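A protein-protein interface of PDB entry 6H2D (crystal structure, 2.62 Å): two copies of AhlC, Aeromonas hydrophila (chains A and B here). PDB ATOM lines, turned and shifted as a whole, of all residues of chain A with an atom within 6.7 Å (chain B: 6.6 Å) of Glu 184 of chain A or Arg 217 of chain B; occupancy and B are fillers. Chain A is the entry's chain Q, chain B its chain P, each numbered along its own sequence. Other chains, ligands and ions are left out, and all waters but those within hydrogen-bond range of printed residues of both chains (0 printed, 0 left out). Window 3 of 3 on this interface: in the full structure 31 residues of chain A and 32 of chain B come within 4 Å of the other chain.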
ATOM      1  N   LEU A 138      -0.091 -31.167   0.881  1.00  0.00           N
ATOM      2  CA  LEU A 138      -0.015 -30.025   1.866  1.00  0.00           C
ATOM      3  C   LEU A 138      -0.676 -28.767   1.279  1.00  0.00           C
ATOM      4  O   LEU A 138      -1.479 -28.112   1.956  1.00  0.00           O
ATOM      5  CB  LEU A 138       1.439 -29.738   2.243  1.00  0.00           C
ATOM      6  CG  LEU A 138       1.739 -28.409   2.952  1.00  0.00           C
ATOM      7  CD1 LEU A 138       0.934 -28.248   4.235  1.00  0.00           C
ATOM      8  CD2 LEU A 138       3.226 -28.296   3.267  1.00  0.00           C
ATOM      9  N   ARG A 142      -3.683 -26.885   2.868  1.00  0.00           N
ATOM     10  CA  ARG A 142      -3.309 -25.517   3.283  1.00  0.00           C
ATOM     11  C   ARG A 142      -4.226 -24.491   2.598  1.00  0.00           C
ATOM     12  O   ARG A 142      -4.414 -23.371   3.099  1.00  0.00           O
ATOM     13  CB  ARG A 142      -1.826 -25.268   2.985  1.00  0.00           C
ATOM     14  CG  ARG A 142      -1.208 -24.092   3.730  1.00  0.00           C
ATOM     15  CD  ARG A 142       0.298 -24.221   3.936  1.00  0.00           C
ATOM     16  NE  ARG A 142       0.932 -24.861   2.797  1.00  0.00           N
ATOM     17  CZ  ARG A 142       2.229 -24.848   2.528  1.00  0.00           C
ATOM     18  NH1 ARG A 142       3.078 -24.200   3.313  1.00  0.00           N
ATOM     19  NH2 ARG A 142       2.655 -25.492   1.454  1.00  0.00           N
ATOM     20  N   LEU A 145      -7.530 -25.095   4.629  1.00  0.00           N
ATOM     21  CA  LEU A 145      -7.455 -24.313   5.888  1.00  0.00           C
ATOM     22  C   LEU A 145      -7.887 -22.863   5.619  1.00  0.00           C
ATOM     23  O   LEU A 145      -8.710 -22.318   6.379  1.00  0.00           O
ATOM     24  CB  LEU A 145      -6.034 -24.389   6.474  1.00  0.00           C
ATOM     25  CG  LEU A 145      -5.801 -23.712   7.836  1.00  0.00           C
ATOM     26  CD1 LEU A 145      -6.808 -24.179   8.892  1.00  0.00           C
ATOM     27  CD2 LEU A 145      -4.373 -23.934   8.335  1.00  0.00           C
ATOM     28  N   ASN A 178      -4.091 -30.034  12.371  1.00  0.00           N
ATOM     29  CA  ASN A 178      -3.112 -31.105  12.700  1.00  0.00           C
ATOM     30  C   ASN A 178      -2.416 -31.620  11.432  1.00  0.00           C
ATOM     31  O   ASN A 178      -1.202 -31.586  11.364  1.00  0.00           O
ATOM     32  CB  ASN A 178      -3.727 -32.268  13.480  1.00  0.00           C
ATOM     33  CG  ASN A 178      -3.911 -31.946  14.944  1.00  0.00           C
ATOM     34  OD1 ASN A 178      -2.946 -31.647  15.654  1.00  0.00           O
ATOM     35  ND2 ASN A 178      -5.156 -31.996  15.389  1.00  0.00           N
ATOM     36  N   LYS A 179      -3.193 -32.095  10.453  1.00  0.00           N
ATOM     37  CA  LYS A 179      -2.632 -32.545   9.192  1.00  0.00           C
ATOM     38  C   LYS A 179      -1.646 -31.481   8.671  1.00  0.00           C
ATOM     39  O   LYS A 179      -0.458 -31.801   8.430  1.00  0.00           O
ATOM     40  CB  LYS A 179      -3.737 -32.864   8.182  1.00  0.00           C
ATOM     41  CG  LYS A 179      -4.278 -34.286   8.249  1.00  0.00           C
ATOM     42  CD  LYS A 179      -5.369 -34.557   7.215  1.00  0.00           C
ATOM     43  CE  LYS A 179      -6.509 -35.429   7.713  1.00  0.00           C
ATOM     44  NZ  LYS A 179      -7.721 -35.284   6.865  1.00  0.00           N
ATOM     45  N   VAL A 180      -2.086 -30.218   8.525  1.00  0.00           N
ATOM     46  CA  VAL A 180      -1.165 -29.269   7.955  1.00  0.00           C
ATOM     47  C   VAL A 180       0.051 -29.157   8.877  1.00  0.00           C
ATOM     48  O   VAL A 180       1.147 -29.067   8.347  1.00  0.00           O
ATOM     49  CB  VAL A 180      -1.751 -27.896   7.596  1.00  0.00           C
ATOM     50  CG1 VAL A 180      -3.126 -28.034   6.986  1.00  0.00           C
ATOM     51  CG2 VAL A 180      -1.725 -26.937   8.768  1.00  0.00           C
ATOM     52  N   SER A 181      -0.132 -29.220  10.210  1.00  0.00           N
ATOM     53  CA  SER A 181       1.015 -29.211  11.171  1.00  0.00           C
ATOM     54  C   SER A 181       2.068 -30.248  10.759  1.00  0.00           C
ATOM     55  O   SER A 181       3.258 -29.924  10.562  1.00  0.00           O
ATOM     56  CB  SER A 181       0.574 -29.447  12.595  1.00  0.00           C
ATOM     57  OG  SER A 181       1.627 -30.022  13.407  1.00  0.00           O
ATOM     58  N   SER A 182       1.619 -31.502  10.603  1.00  0.00           N
ATOM     59  CA  SER A 182       2.506 -32.594  10.297  1.00  0.00           C
ATOM     60  C   SER A 182       3.105 -32.391   8.896  1.00  0.00           C
ATOM     61  O   SER A 182       4.337 -32.193   8.770  1.00  0.00           O
ATOM     62  CB  SER A 182       1.805 -33.908  10.430  1.00  0.00           C
ATOM     63  OG  SER A 182       1.016 -34.162   9.279  1.00  0.00           O
ATOM     64  N   LEU A 183       2.245 -32.397   7.863  1.00  0.00           N
ATOM     65  CA  LEU A 183       2.712 -32.199   6.491  1.00  0.00           C
ATOM     66  C   LEU A 183       3.742 -31.058   6.483  1.00  0.00           C
ATOM     67  O   LEU A 183       4.885 -31.232   6.035  1.00  0.00           O
ATOM     68  CB  LEU A 183       1.530 -31.924   5.559  1.00  0.00           C
ATOM     69  CG  LEU A 183       0.647 -33.138   5.217  1.00  0.00           C
ATOM     70  CD1 LEU A 183      -0.289 -32.814   4.057  1.00  0.00           C
ATOM     71  CD2 LEU A 183       1.467 -34.379   4.886  1.00  0.00           C
ATOM     72  N   GLU A 184       3.380 -29.926   7.084  1.00  0.00           N
ATOM     73  CA  GLU A 184       4.257 -28.795   7.186  1.00  0.00           C
ATOM     74  C   GLU A 184       5.585 -29.157   7.861  1.00  0.00           C
ATOM     75  O   GLU A 184       6.627 -28.706   7.406  1.00  0.00           O
ATOM     76  CB  GLU A 184       3.593 -27.719   8.024  1.00  0.00           C
ATOM     77  CG  GLU A 184       4.222 -26.356   7.899  1.00  0.00           C
ATOM     78  CD  GLU A 184       3.235 -25.321   8.385  1.00  0.00           C
ATOM     79  OE1 GLU A 184       3.563 -24.599   9.343  1.00  0.00           O
ATOM     80  OE2 GLU A 184       2.114 -25.291   7.826  1.00  0.00           O
ATOM     81  N   GLY A 185       5.533 -29.886   8.990  1.00  0.00           N
ATOM     82  CA  GLY A 185       6.738 -30.296   9.704  1.00  0.00           C
ATOM     83  C   GLY A 185       7.557 -31.264   8.866  1.00  0.00           C
ATOM     84  O   GLY A 185       8.771 -31.070   8.648  1.00  0.00           O
ATOM     85  N   GLN A 186       6.882 -32.281   8.319  1.00  0.00           N
ATOM     86  CA  GLN A 186       7.548 -33.232   7.434  1.00  0.00           C
ATOM     87  C   GLN A 186       8.313 -32.495   6.318  1.00  0.00           C
ATOM     88  O   GLN A 186       9.492 -32.680   6.153  1.00  0.00           O
ATOM     89  CB  GLN A 186       6.544 -34.203   6.830  1.00  0.00           C
ATOM     90  CG  GLN A 186       6.079 -35.293   7.779  1.00  0.00           C
ATOM     91  CD  GLN A 186       5.569 -36.449   6.956  1.00  0.00           C
ATOM     92  OE1 GLN A 186       4.378 -36.567   6.683  1.00  0.00           O
ATOM     93  NE2 GLN A 186       6.494 -37.258   6.460  1.00  0.00           N
ATOM     94  N   VAL A 187       7.632 -31.630   5.561  1.00  0.00           N
ATOM     95  CA  VAL A 187       8.300 -30.917   4.473  1.00  0.00           C
ATOM     96  C   VAL A 187       9.453 -30.079   5.049  1.00  0.00           C
ATOM     97  O   VAL A 187      10.540 -30.072   4.503  1.00  0.00           O
ATOM     98  CB  VAL A 187       7.323 -30.096   3.605  1.00  0.00           C
ATOM     99  CG1 VAL A 187       6.316 -30.996   2.897  1.00  0.00           C
ATOM    100  CG2 VAL A 187       6.607 -29.005   4.385  1.00  0.00           C
ATOM    101  N   ASN A 188       9.254 -29.442   6.195  1.00  0.00           N
ATOM    102  CA  ASN A 188      10.240 -28.495   6.697  1.00  0.00           C
ATOM    103  C   ASN A 188      11.480 -29.265   7.140  1.00  0.00           C
ATOM    104  O   ASN A 188      12.586 -28.716   7.160  1.00  0.00           O
ATOM    105  CB  ASN A 188       9.702 -27.647   7.854  1.00  0.00           C
ATOM    106  CG  ASN A 188      10.674 -26.574   8.291  1.00  0.00           C
ATOM    107  OD1 ASN A 188      11.491 -26.793   9.184  1.00  0.00           O
ATOM    108  ND2 ASN A 188      10.607 -25.416   7.648  1.00  0.00           N
ATOM    109  N   GLN A 189      11.280 -30.539   7.511  1.00  0.00           N
ATOM    110  CA  GLN A 189      12.390 -31.436   7.859  1.00  0.00           C
ATOM    111  C   GLN A 189      13.164 -31.802   6.588  1.00  0.00           C
ATOM    112  O   GLN A 189      14.387 -31.659   6.583  1.00  0.00           O
ATOM    113  CB  GLN A 189      11.877 -32.678   8.584  1.00  0.00           C
ATOM    114  CG  GLN A 189      12.949 -33.445   9.337  1.00  0.00           C
ATOM    115  CD  GLN A 189      12.316 -34.672   9.943  1.00  0.00           C
ATOM    116  OE1 GLN A 189      11.532 -35.368   9.293  1.00  0.00           O
ATOM    117  NE2 GLN A 189      12.615 -34.924  11.211  1.00  0.00           N
ATOM    118  N   GLU A 191      13.529 -30.230   4.028  1.00  0.00           N
ATOM    119  CA  GLU A 191      14.285 -28.985   3.701  1.00  0.00           C
ATOM    120  C   GLU A 191      15.633 -28.957   4.405  1.00  0.00           C
ATOM    121  O   GLU A 191      16.712 -28.791   3.755  1.00  0.00           O
ATOM    122  CB  GLU A 191      13.615 -27.735   4.225  1.00  0.00           C
ATOM    123  CG  GLU A 191      12.648 -27.037   3.272  1.00  0.00           C
ATOM    124  CD  GLU A 191      12.326 -25.656   3.852  1.00  0.00           C
ATOM    125  OE1 GLU A 191      13.273 -24.843   3.991  1.00  0.00           O
ATOM    126  OE2 GLU A 191      11.176 -25.440   4.283  1.00  0.00           O
ATOM    127  N   ILE B   5       7.809 -27.583  14.016  1.00  0.00           N
ATOM    128  CA  ILE B   5       8.388 -26.444  13.194  1.00  0.00           C
ATOM    129  C   ILE B   5       9.286 -25.533  14.049  1.00  0.00           C
ATOM    130  O   ILE B   5      10.400 -25.265  13.635  1.00  0.00           O
ATOM    131  CB  ILE B   5       7.326 -25.600  12.456  1.00  0.00           C
ATOM    132  CG1 ILE B   5       6.478 -26.446  11.507  1.00  0.00           C
ATOM    133  CG2 ILE B   5       7.984 -24.455  11.699  1.00  0.00           C
ATOM    134  CD1 ILE B   5       7.167 -26.779  10.188  1.00  0.00           C
ATOM    135  N   LEU B   6       8.797 -25.021  15.189  1.00  0.00           N
ATOM    136  CA  LEU B   6       9.686 -24.350  16.147  1.00  0.00           C
ATOM    137  C   LEU B   6      10.916 -25.215  16.345  1.00  0.00           C
ATOM    138  O   LEU B   6      12.045 -24.771  16.150  1.00  0.00           O
ATOM    139  CB  LEU B   6       9.029 -24.198  17.516  1.00  0.00           C
ATOM    140  CG  LEU B   6       8.232 -22.933  17.729  1.00  0.00           C
ATOM    141  CD1 LEU B   6       7.603 -22.955  19.108  1.00  0.00           C
ATOM    142  CD2 LEU B   6       9.104 -21.712  17.525  1.00  0.00           C
ATOM    143  N   GLN B   8      12.051 -27.983  14.883  1.00  0.00           N
ATOM    144  CA  GLN B   8      12.895 -28.340  13.744  1.00  0.00           C
ATOM    145  C   GLN B   8      13.748 -27.156  13.336  1.00  0.00           C
ATOM    146  O   GLN B   8      14.892 -27.338  12.949  1.00  0.00           O
ATOM    147  CB  GLN B   8      12.092 -28.731  12.505  1.00  0.00           C
ATOM    148  CG  GLN B   8      12.088 -30.221  12.174  1.00  0.00           C
ATOM    149  CD  GLN B   8      11.000 -30.442  11.155  1.00  0.00           C
ATOM    150  OE1 GLN B   8      10.731 -29.564  10.326  1.00  0.00           O
ATOM    151  NE2 GLN B   8      10.336 -31.591  11.231  1.00  0.00           N
ATOM    152  N   SER B   9      13.133 -25.968  13.356  1.00  0.00           N
ATOM    153  CA  SER B   9      13.842 -24.706  13.186  1.00  0.00           C
ATOM    154  C   SER B   9      15.034 -24.681  14.123  1.00  0.00           C
ATOM    155  O   SER B   9      16.148 -24.545  13.658  1.00  0.00           O
ATOM    156  CB  SER B   9      12.967 -23.512  13.431  1.00  0.00           C
ATOM    157  OG  SER B   9      12.008 -23.401  12.394  1.00  0.00           O
ATOM    158  N   GLY B 212      14.227 -17.517  10.099  1.00  0.00           N
ATOM    159  CA  GLY B 212      13.068 -16.849   9.556  1.00  0.00           C
ATOM    160  C   GLY B 212      11.838 -17.680   9.809  1.00  0.00           C
ATOM    161  O   GLY B 212      10.824 -17.171  10.301  1.00  0.00           O
ATOM    162  N   SER B 213      11.954 -18.989   9.536  1.00  0.00           N
ATOM    163  CA  SER B 213      10.897 -19.923   9.858  1.00  0.00           C
ATOM    164  C   SER B 213      10.587 -19.823  11.359  1.00  0.00           C
ATOM    165  O   SER B 213       9.400 -19.758  11.770  1.00  0.00           O
ATOM    166  CB  SER B 213      11.248 -21.292   9.434  1.00  0.00           C
ATOM    167  OG  SER B 213      10.968 -21.488   8.051  1.00  0.00           O
ATOM    168  N   LEU B 214      11.635 -19.707  12.184  1.00  0.00           N
ATOM    169  CA  LEU B 214      11.411 -19.547  13.620  1.00  0.00           C
ATOM    170  C   LEU B 214      10.692 -18.234  13.943  1.00  0.00           C
ATOM    171  O   LEU B 214       9.897 -18.223  14.826  1.00  0.00           O
ATOM    172  CB  LEU B 214      12.729 -19.633  14.383  1.00  0.00           C
ATOM    173  CG  LEU B 214      12.578 -19.743  15.898  1.00  0.00           C
ATOM    174  CD1 LEU B 214      13.810 -20.376  16.476  1.00  0.00           C
ATOM    175  CD2 LEU B 214      12.355 -18.380  16.536  1.00  0.00           C
ATOM    176  N   ILE B 215      10.965 -17.145  13.223  1.00  0.00           N
ATOM    177  CA  ILE B 215      10.378 -15.815  13.556  1.00  0.00           C
ATOM    178  C   ILE B 215       8.911 -15.763  13.070  1.00  0.00           C
ATOM    179  O   ILE B 215       8.067 -15.163  13.710  1.00  0.00           O
ATOM    180  CB  ILE B 215      11.252 -14.685  12.947  1.00  0.00           C
ATOM    181  CG1 ILE B 215      12.545 -14.475  13.721  1.00  0.00           C
ATOM    182  CG2 ILE B 215      10.511 -13.361  12.796  1.00  0.00           C
ATOM    183  CD1 ILE B 215      13.652 -14.034  12.827  1.00  0.00           C
ATOM    184  N   ASP B 216       8.614 -16.390  11.923  1.00  0.00           N
ATOM    185  CA  ASP B 216       7.236 -16.533  11.467  1.00  0.00           C
ATOM    186  C   ASP B 216       6.401 -17.221  12.559  1.00  0.00           C
ATOM    187  O   ASP B 216       5.313 -16.730  12.931  1.00  0.00           O
ATOM    188  CB  ASP B 216       7.125 -17.313  10.156  1.00  0.00           C
ATOM    189  CG  ASP B 216       7.642 -16.606   8.906  1.00  0.00           C
ATOM    190  OD1 ASP B 216       8.057 -15.387   9.003  1.00  0.00           O
ATOM    191  OD2 ASP B 216       7.640 -17.291   7.812  1.00  0.00           O
ATOM    192  N   ARG B 217       6.885 -18.354  13.087  1.00  0.00           N
ATOM    193  CA  ARG B 217       6.072 -19.111  14.020  1.00  0.00           C
ATOM    194  C   ARG B 217       6.011 -18.362  15.351  1.00  0.00           C
ATOM    195  O   ARG B 217       4.925 -18.295  15.944  1.00  0.00           O
ATOM    196  CB  ARG B 217       6.561 -20.553  14.161  1.00  0.00           C
ATOM    197  CG  ARG B 217       5.661 -21.456  14.992  1.00  0.00           C
ATOM    198  CD  ARG B 217       4.211 -21.522  14.536  1.00  0.00           C
ATOM    199  NE  ARG B 217       4.064 -21.743  13.097  1.00  0.00           N
ATOM    200  CZ  ARG B 217       3.775 -22.916  12.523  1.00  0.00           C
ATOM    201  NH1 ARG B 217       3.772 -24.046  13.224  1.00  0.00           N
ATOM    202  NH2 ARG B 217       3.473 -22.931  11.234  1.00  0.00           N
ATOM    203  N   VAL B 218       7.124 -17.744  15.804  1.00  0.00           N
ATOM    204  CA  VAL B 218       7.029 -17.025  17.115  1.00  0.00           C
ATOM    205  C   VAL B 218       5.969 -15.956  16.958  1.00  0.00           C
ATOM    206  O   VAL B 218       5.017 -15.903  17.742  1.00  0.00           O
ATOM    207  CB  VAL B 218       8.312 -16.370  17.626  1.00  0.00           C
ATOM    208  CG1 VAL B 218       7.987 -15.393  18.740  1.00  0.00           C
ATOM    209  CG2 VAL B 218       9.320 -17.404  18.101  1.00  0.00           C
ATOM    210  N   SER B 219       6.160 -15.146  15.904  1.00  0.00           N
ATOM    211  CA  SER B 219       5.227 -14.126  15.504  1.00  0.00           C
ATOM    212  C   SER B 219       3.809 -14.698  15.498  1.00  0.00           C
ATOM    213  O   SER B 219       2.894 -14.071  15.943  1.00  0.00           O
ATOM    214  CB  SER B 219       5.583 -13.557  14.181  1.00  0.00           C
ATOM    215  OG  SER B 219       4.480 -12.846  13.621  1.00  0.00           O
ATOM    216  N   LYS B 220       3.630 -15.896  14.956  1.00  0.00           N
ATOM    217  CA  LYS B 220       2.280 -16.427  14.815  1.00  0.00           C
ATOM    218  C   LYS B 220       1.661 -16.614  16.216  1.00  0.00           C
ATOM    219  O   LYS B 220       0.528 -16.195  16.482  1.00  0.00           O
ATOM    220  CB  LYS B 220       2.320 -17.689  13.952  1.00  0.00           C
ATOM    221  CG  LYS B 220       0.963 -18.057  13.391  1.00  0.00           C
ATOM    222  CD  LYS B 220       0.823 -19.472  12.864  1.00  0.00           C
ATOM    223  CE  LYS B 220      -0.618 -19.822  12.541  1.00  0.00           C
ATOM    224  NZ  LYS B 220      -1.565 -19.299  13.560  1.00  0.00           N
ATOM    225  N   VAL B 221       2.447 -17.176  17.137  1.00  0.00           N
ATOM    226  CA  VAL B 221       2.039 -17.377  18.546  1.00  0.00           C
ATOM    227  C   VAL B 221       1.869 -16.013  19.241  1.00  0.00           C
ATOM    228  O   VAL B 221       0.945 -15.815  19.972  1.00  0.00           O
ATOM    229  CB  VAL B 221       3.040 -18.306  19.280  1.00  0.00           C
ATOM    230  CG1 VAL B 221       2.947 -18.208  20.809  1.00  0.00           C
ATOM    231  CG2 VAL B 221       2.911 -19.751  18.777  1.00  0.00           C
ATOM    232  N   GLY B 222       2.764 -15.061  19.004  1.00  0.00           N
ATOM    233  CA  GLY B 222       2.465 -13.660  19.384  1.00  0.00           C
ATOM    234  C   GLY B 222       1.047 -13.211  18.999  1.00  0.00           C
ATOM    235  O   GLY B 222       0.383 -12.568  19.777  1.00  0.00           O
ATOM    236  N   VAL B 263      -1.524 -26.087  18.702  1.00  0.00           N
ATOM    237  CA  VAL B 263      -1.007 -26.752  17.493  1.00  0.00           C
ATOM    238  C   VAL B 263       0.237 -25.993  16.999  1.00  0.00           C
ATOM    239  O   VAL B 263       1.214 -26.605  16.524  1.00  0.00           O
ATOM    240  CB  VAL B 263      -2.083 -26.873  16.397  1.00  0.00           C
ATOM    241  CG1 VAL B 263      -1.526 -27.416  15.095  1.00  0.00           C
ATOM    242  CG2 VAL B 263      -3.236 -27.748  16.834  1.00  0.00           C
ATOM    243  N   ASP B 264       0.209 -24.663  17.117  1.00  0.00           N
ATOM    244  CA  ASP B 264       1.326 -23.830  16.703  1.00  0.00           C
ATOM    245  C   ASP B 264       2.474 -23.978  17.710  1.00  0.00           C
ATOM    246  O   ASP B 264       3.616 -24.204  17.289  1.00  0.00           O
ATOM    247  CB  ASP B 264       0.881 -22.373  16.489  1.00  0.00           C
ATOM    248  CG  ASP B 264       0.041 -22.153  15.230  1.00  0.00           C
ATOM    249  OD1 ASP B 264       0.296 -22.824  14.220  1.00  0.00           O
ATOM    250  OD2 ASP B 264      -0.865 -21.318  15.267  1.00  0.00           O
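Of the 16 printed residues of chain A, 5 touch a printed residue of chain B. Along chain A the printed residues that touch a printed residue of chain B span positions 181 to 189. Among the printed residues, 9 pairs touch across the chains. Among the printed residues, Asp or Glu carboxylates within 4 Å of a Lys or Arg side-chain nitrogen of the other chain: Glu 184 of chain A with Arg 217 of chain B.
No position is printed for both chains. Of the 9 pairs that touch across the chains among the printed residues, none has its exchanged pair printed and touching as well.
The side-chain amide oxygen of Gln 8 of chain B sits close to the backbone carbonyl oxygen of Gly 185 of chain A (3.0 Å). The side-chain amide oxygen (OD1) of Asn 188 of chain A sits close to the side-chain amide oxygen (OE1) of Gln 8 of chain B. The backbone NH (N) of Gln 189 of chain A is in hydrogen-bond range of the side-chain amide oxygen (OE1) of Gln 8 of chain B (3.0 Å). The guanidinium group (NH2) of Arg 217 of chain B lies within salt-bridge range of the side-chain carboxylate (OE1) of Glu 184 of chain A (2.5 Å).
OG of Ser 9 of chain B sits at hydrogen-bond distance from O of Ile 5 of chain B, 2.8 Å away. NH1 of Arg 217 of chain B is in salt-bridge range of OD1 of Asp 264 of chain B (3.8 Å). The side-chain carboxylate of Glu 191 of chain A sits at hydrogen-bond distance from the side-chain amide nitrogen of Asn 188 of chain A, 3.4 Å away.
Val 263 of chain B touches Ser 181 of chain A. CD1 of Ile 5 of chain B touches O of Glu 184 of chain A, at 3.4 Å. CD1 of Ile 5 of chain B touches CA of Gly 185 of chain A, at 3.6 Å. Asn 188 of chain A touches Ile 5 of chain B (CB to CD1, 3.6 Å). Asn 188 of chain A touches Ser 213 of chain B.
Arg 217 of chain B touches just one residue of chain A: Glu 184. Of the printed residues of chain B, Ser 181 of chain A touches Val 263. Of the printed residues of chain A, Ser 213 of chain B touches Asn 188. Of the printed residues of chain B, Asn 188 of chain A touches Ile 5 (3.6 Å), Gln 8 (3.1 Å) and Ser 213 (3.97 Å). Of the printed residues of chain B, Gly 185 of chain A touches Ile 5 and Gln 8. Of the printed residues of chain B, Gln 189 of chain A touches Gln 8. Val 180 of chain A touches none of the printed residues of chain B. Lys 179 of chain A touches none of the printed residues of chain B. The nearest residue of chain B that does not touch Glu 184 of chain A is Gln 8 of chain B (5.1 Å).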
